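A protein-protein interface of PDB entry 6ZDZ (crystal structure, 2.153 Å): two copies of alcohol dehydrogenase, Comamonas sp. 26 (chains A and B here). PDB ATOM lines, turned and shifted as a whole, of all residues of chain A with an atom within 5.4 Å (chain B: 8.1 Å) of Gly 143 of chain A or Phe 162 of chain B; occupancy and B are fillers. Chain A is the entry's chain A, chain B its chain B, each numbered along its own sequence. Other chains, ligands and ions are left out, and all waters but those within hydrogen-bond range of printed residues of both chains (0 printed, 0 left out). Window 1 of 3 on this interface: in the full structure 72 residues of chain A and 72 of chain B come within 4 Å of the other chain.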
ATOM      1  N   SER A 140      11.810   8.255  -5.248  1.00  0.00           N
ATOM      2  CA  SER A 140      12.134   9.315  -4.302  1.00  0.00           C
ATOM      3  C   SER A 140      13.639   9.333  -4.091  1.00  0.00           C
ATOM      4  O   SER A 140      14.307   8.305  -4.238  1.00  0.00           O
ATOM      5  CB  SER A 140      11.416   9.122  -2.961  1.00  0.00           C
ATOM      6  OG  SER A 140      11.922  10.015  -1.984  1.00  0.00           O
ATOM      7  N   VAL A 141      14.165  10.512  -3.743  1.00  0.00           N
ATOM      8  CA  VAL A 141      15.577  10.623  -3.394  1.00  0.00           C
ATOM      9  C   VAL A 141      15.897   9.960  -2.064  1.00  0.00           C
ATOM     10  O   VAL A 141      17.077   9.764  -1.749  1.00  0.00           O
ATOM     11  CB  VAL A 141      16.030  12.097  -3.356  1.00  0.00           C
ATOM     12  CG1 VAL A 141      15.752  12.772  -4.691  1.00  0.00           C
ATOM     13  CG2 VAL A 141      15.339  12.836  -2.222  1.00  0.00           C
ATOM     14  N   VAL A 142      14.875   9.621  -1.274  1.00  0.00           N
ATOM     15  CA  VAL A 142      15.097   8.863  -0.045  1.00  0.00           C
ATOM     16  C   VAL A 142      15.741   7.520  -0.358  1.00  0.00           C
ATOM     17  O   VAL A 142      16.495   6.976   0.460  1.00  0.00           O
ATOM     18  CB  VAL A 142      13.771   8.698   0.724  1.00  0.00           C
ATOM     19  CG1 VAL A 142      13.994   7.960   2.034  1.00  0.00           C
ATOM     20  CG2 VAL A 142      13.141  10.057   0.986  1.00  0.00           C
ATOM     21  N   GLY A 143      15.474   6.971  -1.544  1.00  0.00           N
ATOM     22  CA  GLY A 143      16.145   5.761  -1.989  1.00  0.00           C
ATOM     23  C   GLY A 143      17.653   5.884  -2.081  1.00  0.00           C
ATOM     24  O   GLY A 143      18.331   4.863  -2.255  1.00  0.00           O
ATOM     25  N   PHE A 144      18.190   7.101  -1.975  1.00  0.00           N
ATOM     26  CA  PHE A 144      19.626   7.330  -1.920  1.00  0.00           C
ATOM     27  C   PHE A 144      20.147   7.579  -0.512  1.00  0.00           C
ATOM     28  O   PHE A 144      21.366   7.664  -0.330  1.00  0.00           O
ATOM     29  CB  PHE A 144      20.017   8.536  -2.785  1.00  0.00           C
ATOM     30  CG  PHE A 144      19.763   8.354  -4.250  1.00  0.00           C
ATOM     31  CD1 PHE A 144      20.073   7.164  -4.883  1.00  0.00           C
ATOM     32  CD2 PHE A 144      19.243   9.393  -5.002  1.00  0.00           C
ATOM     33  CE1 PHE A 144      19.850   7.006  -6.237  1.00  0.00           C
ATOM     34  CE2 PHE A 144      19.022   9.244  -6.353  1.00  0.00           C
ATOM     35  CZ  PHE A 144      19.322   8.048  -6.972  1.00  0.00           C
ATOM     36  N   ALA A 145      19.271   7.703   0.484  1.00  0.00           N
ATOM     37  CA  ALA A 145      19.644   8.228   1.797  1.00  0.00           C
ATOM     38  C   ALA A 145      19.064   7.366   2.909  1.00  0.00           C
ATOM     39  O   ALA A 145      18.008   7.687   3.474  1.00  0.00           O
ATOM     40  CB  ALA A 145      19.194   9.681   1.949  1.00  0.00           C
ATOM     41  N   PRO A 146      19.730   6.261   3.254  1.00  0.00           N
ATOM     42  CA  PRO A 146      19.356   5.530   4.475  1.00  0.00           C
ATOM     43  C   PRO A 146      19.652   6.300   5.752  1.00  0.00           C
ATOM     44  O   PRO A 146      19.232   5.858   6.831  1.00  0.00           O
ATOM     45  CB  PRO A 146      20.197   4.251   4.392  1.00  0.00           C
ATOM     46  CG  PRO A 146      21.363   4.623   3.540  1.00  0.00           C
ATOM     47  CD  PRO A 146      20.840   5.610   2.536  1.00  0.00           C
ATOM     48  N   MET A 150      14.078   6.640   7.257  1.00  0.00           N
ATOM     49  CA  MET A 150      12.888   6.046   6.651  1.00  0.00           C
ATOM     50  C   MET A 150      13.308   4.777   5.915  1.00  0.00           C
ATOM     51  O   MET A 150      13.356   4.720   4.684  1.00  0.00           O
ATOM     52  CB  MET A 150      12.197   7.057   5.725  1.00  0.00           C
ATOM     53  CG  MET A 150      11.649   8.276   6.459  1.00  0.00           C
ATOM     54  SD  MET A 150      11.036   9.568   5.358  1.00  0.00           S
ATOM     55  CE  MET A 150      12.575  10.243   4.738  1.00  0.00           C
ATOM     56  N   THR A 151      13.613   3.744   6.704  1.00  0.00           N
ATOM     57  CA  THR A 151      14.318   2.575   6.185  1.00  0.00           C
ATOM     58  C   THR A 151      13.478   1.813   5.166  1.00  0.00           C
ATOM     59  O   THR A 151      13.923   1.578   4.037  1.00  0.00           O
ATOM     60  CB  THR A 151      14.722   1.660   7.340  1.00  0.00           C
ATOM     61  OG1 THR A 151      15.596   2.370   8.227  1.00  0.00           O
ATOM     62  CG2 THR A 151      15.437   0.426   6.816  1.00  0.00           C
ATOM     63  N   GLY A 154      12.460   4.146   2.059  1.00  0.00           N
ATOM     64  CA  GLY A 154      13.596   4.328   1.173  1.00  0.00           C
ATOM     65  C   GLY A 154      13.993   3.058   0.448  1.00  0.00           C
ATOM     66  O   GLY A 154      14.448   3.109  -0.697  1.00  0.00           O
ATOM     67  N   ALA A 155      13.836   1.907   1.105  1.00  0.00           N
ATOM     68  CA  ALA A 155      14.143   0.637   0.457  1.00  0.00           C
ATOM     69  C   ALA A 155      13.204   0.374  -0.714  1.00  0.00           C
ATOM     70  O   ALA A 155      13.642  -0.080  -1.779  1.00  0.00           O
ATOM     71  CB  ALA A 155      14.077  -0.498   1.479  1.00  0.00           C
ATOM     72  N   LYS A 157      11.811   2.630  -2.474  1.00  0.00           N
ATOM     73  CA  LYS A 157      12.142   3.584  -3.525  1.00  0.00           C
ATOM     74  C   LYS A 157      13.407   3.177  -4.269  1.00  0.00           C
ATOM     75  O   LYS A 157      13.514   3.398  -5.480  1.00  0.00           O
ATOM     76  CB  LYS A 157      12.282   4.987  -2.936  1.00  0.00           C
ATOM     77  CG  LYS A 157      10.975   5.546  -2.402  1.00  0.00           C
ATOM     78  CD  LYS A 157       9.890   5.467  -3.465  1.00  0.00           C
ATOM     79  CE  LYS A 157       8.529   5.844  -2.907  1.00  0.00           C
ATOM     80  NZ  LYS A 157       7.453   5.690  -3.925  1.00  0.00           N
ATOM     81  N   ALA A 158      14.376   2.592  -3.561  1.00  0.00           N
ATOM     82  CA  ALA A 158      15.520   1.995  -4.239  1.00  0.00           C
ATOM     83  C   ALA A 158      15.075   0.855  -5.146  1.00  0.00           C
ATOM     84  O   ALA A 158      15.639   0.655  -6.228  1.00  0.00           O
ATOM     85  CB  ALA A 158      16.543   1.503  -3.215  1.00  0.00           C
ATOM     86  N   ASN B 137      21.482 -10.088   6.326  1.00  0.00           N
ATOM     87  CA  ASN B 137      20.610 -10.095   5.159  1.00  0.00           C
ATOM     88  C   ASN B 137      21.399 -10.553   3.941  1.00  0.00           C
ATOM     89  O   ASN B 137      22.440  -9.971   3.617  1.00  0.00           O
ATOM     90  CB  ASN B 137      20.011  -8.710   4.908  1.00  0.00           C
ATOM     91  CG  ASN B 137      19.068  -8.271   6.010  1.00  0.00           C
ATOM     92  OD1 ASN B 137      18.252  -9.055   6.494  1.00  0.00           O
ATOM     93  ND2 ASN B 137      19.171  -7.008   6.408  1.00  0.00           N
ATOM     94  N   ALA B 155      15.914  -5.807  -8.280  1.00  0.00           N
ATOM     95  CA  ALA B 155      15.234  -4.748  -7.544  1.00  0.00           C
ATOM     96  C   ALA B 155      14.997  -5.148  -6.092  1.00  0.00           C
ATOM     97  O   ALA B 155      15.190  -4.337  -5.179  1.00  0.00           O
ATOM     98  CB  ALA B 155      13.916  -4.394  -8.232  1.00  0.00           C
ATOM     99  N   THR B 156      14.572  -6.394  -5.858  1.00  0.00           N
ATOM    100  CA  THR B 156      14.392  -6.856  -4.485  1.00  0.00           C
ATOM    101  C   THR B 156      15.712  -6.876  -3.728  1.00  0.00           C
ATOM    102  O   THR B 156      15.731  -6.662  -2.511  1.00  0.00           O
ATOM    103  CB  THR B 156      13.760  -8.251  -4.462  1.00  0.00           C
ATOM    104  OG1 THR B 156      14.667  -9.200  -5.038  1.00  0.00           O
ATOM    105  CG2 THR B 156      12.446  -8.264  -5.229  1.00  0.00           C
ATOM    106  N   LYS B 157      16.822  -7.132  -4.423  1.00  0.00           N
ATOM    107  CA  LYS B 157      18.122  -7.156  -3.762  1.00  0.00           C
ATOM    108  C   LYS B 157      18.629  -5.748  -3.471  1.00  0.00           C
ATOM    109  O   LYS B 157      19.279  -5.522  -2.445  1.00  0.00           O
ATOM    110  CB  LYS B 157      19.124  -7.937  -4.609  1.00  0.00           C
ATOM    111  CG  LYS B 157      18.777  -9.412  -4.721  1.00  0.00           C
ATOM    112  CD  LYS B 157      18.568 -10.016  -3.340  1.00  0.00           C
ATOM    113  CE  LYS B 157      18.029 -11.434  -3.424  1.00  0.00           C
ATOM    114  NZ  LYS B 157      17.745 -11.995  -2.074  1.00  0.00           N
ATOM    115  N   ALA B 158      18.351  -4.792  -4.363  1.00  0.00           N
ATOM    116  CA  ALA B 158      18.639  -3.395  -4.049  1.00  0.00           C
ATOM    117  C   ALA B 158      17.834  -2.940  -2.840  1.00  0.00           C
ATOM    118  O   ALA B 158      18.318  -2.152  -2.019  1.00  0.00           O
ATOM    119  CB  ALA B 158      18.349  -2.510  -5.261  1.00  0.00           C
ATOM    120  N   PHE B 159      16.593  -3.421  -2.727  1.00  0.00           N
ATOM    121  CA  PHE B 159      15.804  -3.215  -1.517  1.00  0.00           C
ATOM    122  C   PHE B 159      16.544  -3.747  -0.294  1.00  0.00           C
ATOM    123  O   PHE B 159      16.642  -3.067   0.735  1.00  0.00           O
ATOM    124  CB  PHE B 159      14.441  -3.900  -1.676  1.00  0.00           C
ATOM    125  CG  PHE B 159      13.527  -3.756  -0.486  1.00  0.00           C
ATOM    126  CD1 PHE B 159      13.701  -4.535   0.648  1.00  0.00           C
ATOM    127  CD2 PHE B 159      12.463  -2.871  -0.521  1.00  0.00           C
ATOM    128  CE1 PHE B 159      12.860  -4.408   1.733  1.00  0.00           C
ATOM    129  CE2 PHE B 159      11.612  -2.742   0.564  1.00  0.00           C
ATOM    130  CZ  PHE B 159      11.812  -3.511   1.692  1.00  0.00           C
ATOM    131  N   VAL B 160      17.065  -4.974  -0.390  1.00  0.00           N
ATOM    132  CA  VAL B 160      17.692  -5.624   0.759  1.00  0.00           C
ATOM    133  C   VAL B 160      18.934  -4.860   1.202  1.00  0.00           C
ATOM    134  O   VAL B 160      19.208  -4.737   2.404  1.00  0.00           O
ATOM    135  CB  VAL B 160      18.017  -7.093   0.424  1.00  0.00           C
ATOM    136  CG1 VAL B 160      18.851  -7.727   1.523  1.00  0.00           C
ATOM    137  CG2 VAL B 160      16.737  -7.884   0.221  1.00  0.00           C
ATOM    138  N   LEU B 161      19.700  -4.327   0.247  1.00  0.00           N
ATOM    139  CA  LEU B 161      20.891  -3.563   0.604  1.00  0.00           C
ATOM    140  C   LEU B 161      20.521  -2.286   1.348  1.00  0.00           C
ATOM    141  O   LEU B 161      21.126  -1.957   2.376  1.00  0.00           O
ATOM    142  CB  LEU B 161      21.713  -3.242  -0.644  1.00  0.00           C
ATOM    143  CG  LEU B 161      22.986  -2.436  -0.382  1.00  0.00           C
ATOM    144  CD1 LEU B 161      23.869  -3.144   0.637  1.00  0.00           C
ATOM    145  CD2 LEU B 161      23.746  -2.199  -1.675  1.00  0.00           C
ATOM    146  N   PHE B 162      19.532  -1.546   0.837  1.00  0.00           N
ATOM    147  CA  PHE B 162      19.090  -0.334   1.520  1.00  0.00           C
ATOM    148  C   PHE B 162      18.546  -0.654   2.907  1.00  0.00           C
ATOM    149  O   PHE B 162      18.808   0.079   3.868  1.00  0.00           O
ATOM    150  CB  PHE B 162      18.035   0.389   0.681  1.00  0.00           C
ATOM    151  CG  PHE B 162      17.710   1.776   1.172  1.00  0.00           C
ATOM    152  CD1 PHE B 162      16.866   1.967   2.257  1.00  0.00           C
ATOM    153  CD2 PHE B 162      18.245   2.889   0.546  1.00  0.00           C
ATOM    154  CE1 PHE B 162      16.567   3.238   2.706  1.00  0.00           C
ATOM    155  CE2 PHE B 162      17.948   4.162   0.992  1.00  0.00           C
ATOM    156  CZ  PHE B 162      17.108   4.336   2.072  1.00  0.00           C
ATOM    157  N   LEU B 163      17.771  -1.736   3.026  1.00  0.00           N
ATOM    158  CA  LEU B 163      17.255  -2.142   4.330  1.00  0.00           C
ATOM    159  C   LEU B 163      18.385  -2.372   5.323  1.00  0.00           C
ATOM    160  O   LEU B 163      18.306  -1.935   6.477  1.00  0.00           O
ATOM    161  CB  LEU B 163      16.402  -3.402   4.186  1.00  0.00           C
ATOM    162  CG  LEU B 163      15.855  -3.999   5.484  1.00  0.00           C
ATOM    163  CD1 LEU B 163      14.696  -3.170   6.014  1.00  0.00           C
ATOM    164  CD2 LEU B 163      15.435  -5.447   5.276  1.00  0.00           C
ATOM    165  N   SER B 164      19.449  -3.055   4.891  1.00  0.00           N
ATOM    166  CA  SER B 164      20.577  -3.312   5.781  1.00  0.00           C
ATOM    167  C   SER B 164      21.262  -2.016   6.195  1.00  0.00           C
ATOM    168  O   SER B 164      21.612  -1.837   7.368  1.00  0.00           O
ATOM    169  CB  SER B 164      21.573  -4.251   5.105  1.00  0.00           C
ATOM    170  OG  SER B 164      20.961  -5.485   4.769  1.00  0.00           O
ATOM    171  N   GLN B 165      21.469  -1.102   5.243  1.00  0.00           N
ATOM    172  CA  GLN B 165      22.104   0.173   5.563  1.00  0.00           C
ATOM    173  C   GLN B 165      21.254   0.991   6.526  1.00  0.00           C
ATOM    174  O   GLN B 165      21.778   1.604   7.463  1.00  0.00           O
ATOM    175  CB  GLN B 165      22.374   0.960   4.281  1.00  0.00           C
ATOM    176  CG  GLN B 165      23.394   0.311   3.358  1.00  0.00           C
ATOM    177  CD  GLN B 165      23.507   1.022   2.023  1.00  0.00           C
ATOM    178  OE1 GLN B 165      22.537   1.108   1.267  1.00  0.00           O
ATOM    179  NE2 GLN B 165      24.695   1.539   1.728  1.00  0.00           N
ATOM    180  N   GLY B 166      19.937   1.018   6.309  1.00  0.00           N
ATOM    181  CA  GLY B 166      19.066   1.750   7.214  1.00  0.00           C
ATOM    182  C   GLY B 166      18.976   1.112   8.587  1.00  0.00           C
ATOM    183  O   GLY B 166      18.993   1.807   9.607  1.00  0.00           O
ATOM    184  N   LEU B 167      18.875  -0.220   8.635  1.00  0.00           N
ATOM    185  CA  LEU B 167      18.802  -0.907   9.920  1.00  0.00           C
ATOM    186  C   LEU B 167      20.093  -0.759  10.713  1.00  0.00           C
ATOM    187  O   LEU B 167      20.057  -0.717  11.948  1.00  0.00           O
ATOM    188  CB  LEU B 167      18.471  -2.385   9.712  1.00  0.00           C
ATOM    189  CG  LEU B 167      17.024  -2.685   9.316  1.00  0.00           C
ATOM    190  CD1 LEU B 167      16.789  -4.184   9.201  1.00  0.00           C
ATOM    191  CD2 LEU B 167      16.064  -2.058  10.312  1.00  0.00           C
ATOM    192  N   ASN B 168      21.237  -0.692  10.029  1.00  0.00           N
ATOM    193  CA  ASN B 168      22.500  -0.459  10.723  1.00  0.00           C
ATOM    194  C   ASN B 168      22.493   0.890  11.433  1.00  0.00           C
ATOM    195  O   ASN B 168      22.838   0.983  12.616  1.00  0.00           O
ATOM    196  CB  ASN B 168      23.664  -0.542   9.736  1.00  0.00           C
ATOM    197  CG  ASN B 168      24.962  -0.025  10.326  1.00  0.00           C
ATOM    198  OD1 ASN B 168      25.495   0.994   9.885  1.00  0.00           O
ATOM    199  ND2 ASN B 168      25.468  -0.718  11.340  1.00  0.00           N
ATOM    200  N   LEU B 169      22.107   1.951  10.720  1.00  0.00           N
ATOM    201  CA  LEU B 169      22.097   3.278  11.325  1.00  0.00           C
ATOM    202  C   LEU B 169      21.037   3.398  12.413  1.00  0.00           C
ATOM    203  O   LEU B 169      21.182   4.217  13.328  1.00  0.00           O
ATOM    204  CB  LEU B 169      21.877   4.341  10.251  1.00  0.00           C
ATOM    205  CG  LEU B 169      22.948   4.406   9.159  1.00  0.00           C
ATOM    206  CD1 LEU B 169      22.644   5.525   8.179  1.00  0.00           C
ATOM    207  CD2 LEU B 169      24.328   4.590   9.772  1.00  0.00           C
ATOM    208  N   VAL B 178      24.060  -5.434  11.994  1.00  0.00           N
ATOM    209  CA  VAL B 178      23.304  -5.684  10.771  1.00  0.00           C
ATOM    210  C   VAL B 178      24.291  -5.788   9.619  1.00  0.00           C
ATOM    211  O   VAL B 178      24.962  -4.806   9.280  1.00  0.00           O
ATOM    212  CB  VAL B 178      22.263  -4.584  10.506  1.00  0.00           C
ATOM    213  CG1 VAL B 178      21.481  -4.890   9.238  1.00  0.00           C
ATOM    214  CG2 VAL B 178      21.325  -4.437  11.698  1.00  0.00           C
ATOM    215  N   ALA B 180      25.092  -6.966   5.531  1.00  0.00           N
ATOM    216  CA  ALA B 180      24.609  -7.255   4.188  1.00  0.00           C
ATOM    217  C   ALA B 180      25.647  -8.108   3.471  1.00  0.00           C
ATOM    218  O   ALA B 180      26.788  -7.674   3.279  1.00  0.00           O
ATOM    219  CB  ALA B 180      24.338  -5.966   3.411  1.00  0.00           C
ATOM    220  N   TRP B 235      33.352  -0.468  -3.529  1.00  0.00           N
ATOM    221  CA  TRP B 235      32.154  -0.270  -2.719  1.00  0.00           C
ATOM    222  C   TRP B 235      32.187   1.076  -2.008  1.00  0.00           C
ATOM    223  O   TRP B 235      31.202   1.825  -2.028  1.00  0.00           O
ATOM    224  CB  TRP B 235      31.996  -1.405  -1.709  1.00  0.00           C
ATOM    225  CG  TRP B 235      31.039  -1.058  -0.613  1.00  0.00           C
ATOM    226  CD1 TRP B 235      31.319  -0.954   0.719  1.00  0.00           C
ATOM    227  CD2 TRP B 235      29.653  -0.725  -0.758  1.00  0.00           C
ATOM    228  NE1 TRP B 235      30.188  -0.599   1.414  1.00  0.00           N
ATOM    229  CE2 TRP B 235      29.152  -0.450   0.530  1.00  0.00           C
ATOM    230  CE3 TRP B 235      28.784  -0.643  -1.850  1.00  0.00           C
ATOM    231  CZ2 TRP B 235      27.823  -0.098   0.754  1.00  0.00           C
ATOM    232  CZ3 TRP B 235      27.466  -0.293  -1.626  1.00  0.00           C
ATOM    233  CH2 TRP B 235      26.997  -0.026  -0.333  1.00  0.00           C
ATOM    234  N   ARG B 242      27.146   7.967  -3.797  1.00  0.00           N
ATOM    235  CA  ARG B 242      25.767   8.083  -3.338  1.00  0.00           C
ATOM    236  C   ARG B 242      25.587   9.299  -2.438  1.00  0.00           C
ATOM    237  O   ARG B 242      24.681  10.114  -2.646  1.00  0.00           O
ATOM    238  CB  ARG B 242      25.356   6.808  -2.603  1.00  0.00           C
ATOM    239  CG  ARG B 242      23.919   6.812  -2.118  1.00  0.00           C
ATOM    240  CD  ARG B 242      23.643   5.618  -1.225  1.00  0.00           C
ATOM    241  NE  ARG B 242      24.563   5.573  -0.090  1.00  0.00           N
ATOM    242  CZ  ARG B 242      24.421   6.292   1.019  1.00  0.00           C
ATOM    243  NH1 ARG B 242      23.394   7.122   1.151  1.00  0.00           N
ATOM    244  NH2 ARG B 242      25.310   6.185   1.997  1.00  0.00           N
ATOM    245  N   MET B 246      23.375  13.202  -2.640  1.00  0.00           N
ATOM    246  CA  MET B 246      22.500  13.803  -1.642  1.00  0.00           C
ATOM    247  C   MET B 246      22.995  15.167  -1.184  1.00  0.00           C
ATOM    248  O   MET B 246      22.186  15.983  -0.728  1.00  0.00           O
ATOM    249  CB  MET B 246      22.350  12.868  -0.440  1.00  0.00           C
ATOM    250  CG  MET B 246      21.516  11.628  -0.722  1.00  0.00           C
ATOM    251  SD  MET B 246      19.843  12.028  -1.265  1.00  0.00           S
ATOM    252  CE  MET B 246      19.257  13.000   0.121  1.00  0.00           C
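OG of Ser 140 of chain A is in hydrogen-bond range of N of Val 142 of chain A (3.1 Å).
The backbone carbonyl oxygen (O) of Phe 144 of chain A lies within hydrogen-bond range of the guanidinium group (NH1) of Arg 242 of chain B.
The backbone carbonyl oxygen (O) of Val 141 of chain A sits close to the side-chain sulfur (SD) of Met 246 of chain B, at 3.6 Å.
Positions printed for both chains: 155, 157 and 158.
Of the 21 printed residues of chain B, 9 touch a printed residue of chain A.
Hydrophobic or aromatic side chains of chain B within 4 Å of the printed part of chain A: Phe 159, Phe 162, Leu 163, Leu 169 and Met 246.
Among the printed residues, no Asp or Glu carboxylate lies within 4 Å of a Lys or Arg side-chain nitrogen of the other chain.
Gly 143 of chain A touches just one residue of chain B: Phe 162.
Phe 162 of chain B touches just these residues of chain A: Val 142, Gly 143, Ala 145, Pro 146, Thr 151, Gly 154 and Ala 155.
Printed residues of chain A within 4 Å of Phe 159 of chain B: Ala 155 (3.3 Å).
Printed residues of chain A within 4 Å of Arg 242 of chain B: Phe 144 (2.6 Å), Ala 145 (3.96 Å) and Pro 146 (3.3 Å).
Printed residues of chain B within 4 Å of Phe 144 of chain A: Arg 242 (2.6 Å) and Met 246 (3.8 Å).
Of the printed residues of chain A, Leu 169 of chain B touches Pro 146.
Lys 157 of chain B touches none of the printed residues of chain A.
Ala 158 of chain A touches none of the printed residues of chain B.
The nearest printed residue of chain A that does not touch Gln 165 of chain B is Thr 151 of chain A (5.9 Å).
Val 142 of chain A touches Phe 162 of chain B (O to CZ, 3.2 Å).
C of Ala 145 of chain A touches CZ of Phe 162 of chain B, at 3.7 Å.
Ala 145 of chain A touches Arg 242 of chain B (CA to NH1, 3.96 Å).
Ala 145 of chain A touches Met 246 of chain B (CB to CE, 3.8 Å).
N of Pro 146 of chain A touches CZ of Phe 162 of chain B, 3.5 Å away.
Pro 146 of chain A touches Gln 165 of chain B.
Pro 146 of chain A touches Gly 166 of chain B.
C of Gly 166 of chain B touches OG1 of Thr 151 of chain A, 3.6 Å away.
N of Leu 167 of chain B touches CG2 of Thr 151 of chain A, at 3.9 Å.
Ala 155 of chain A touches Phe 159 of chain B (O to CD2, 3.3 Å).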
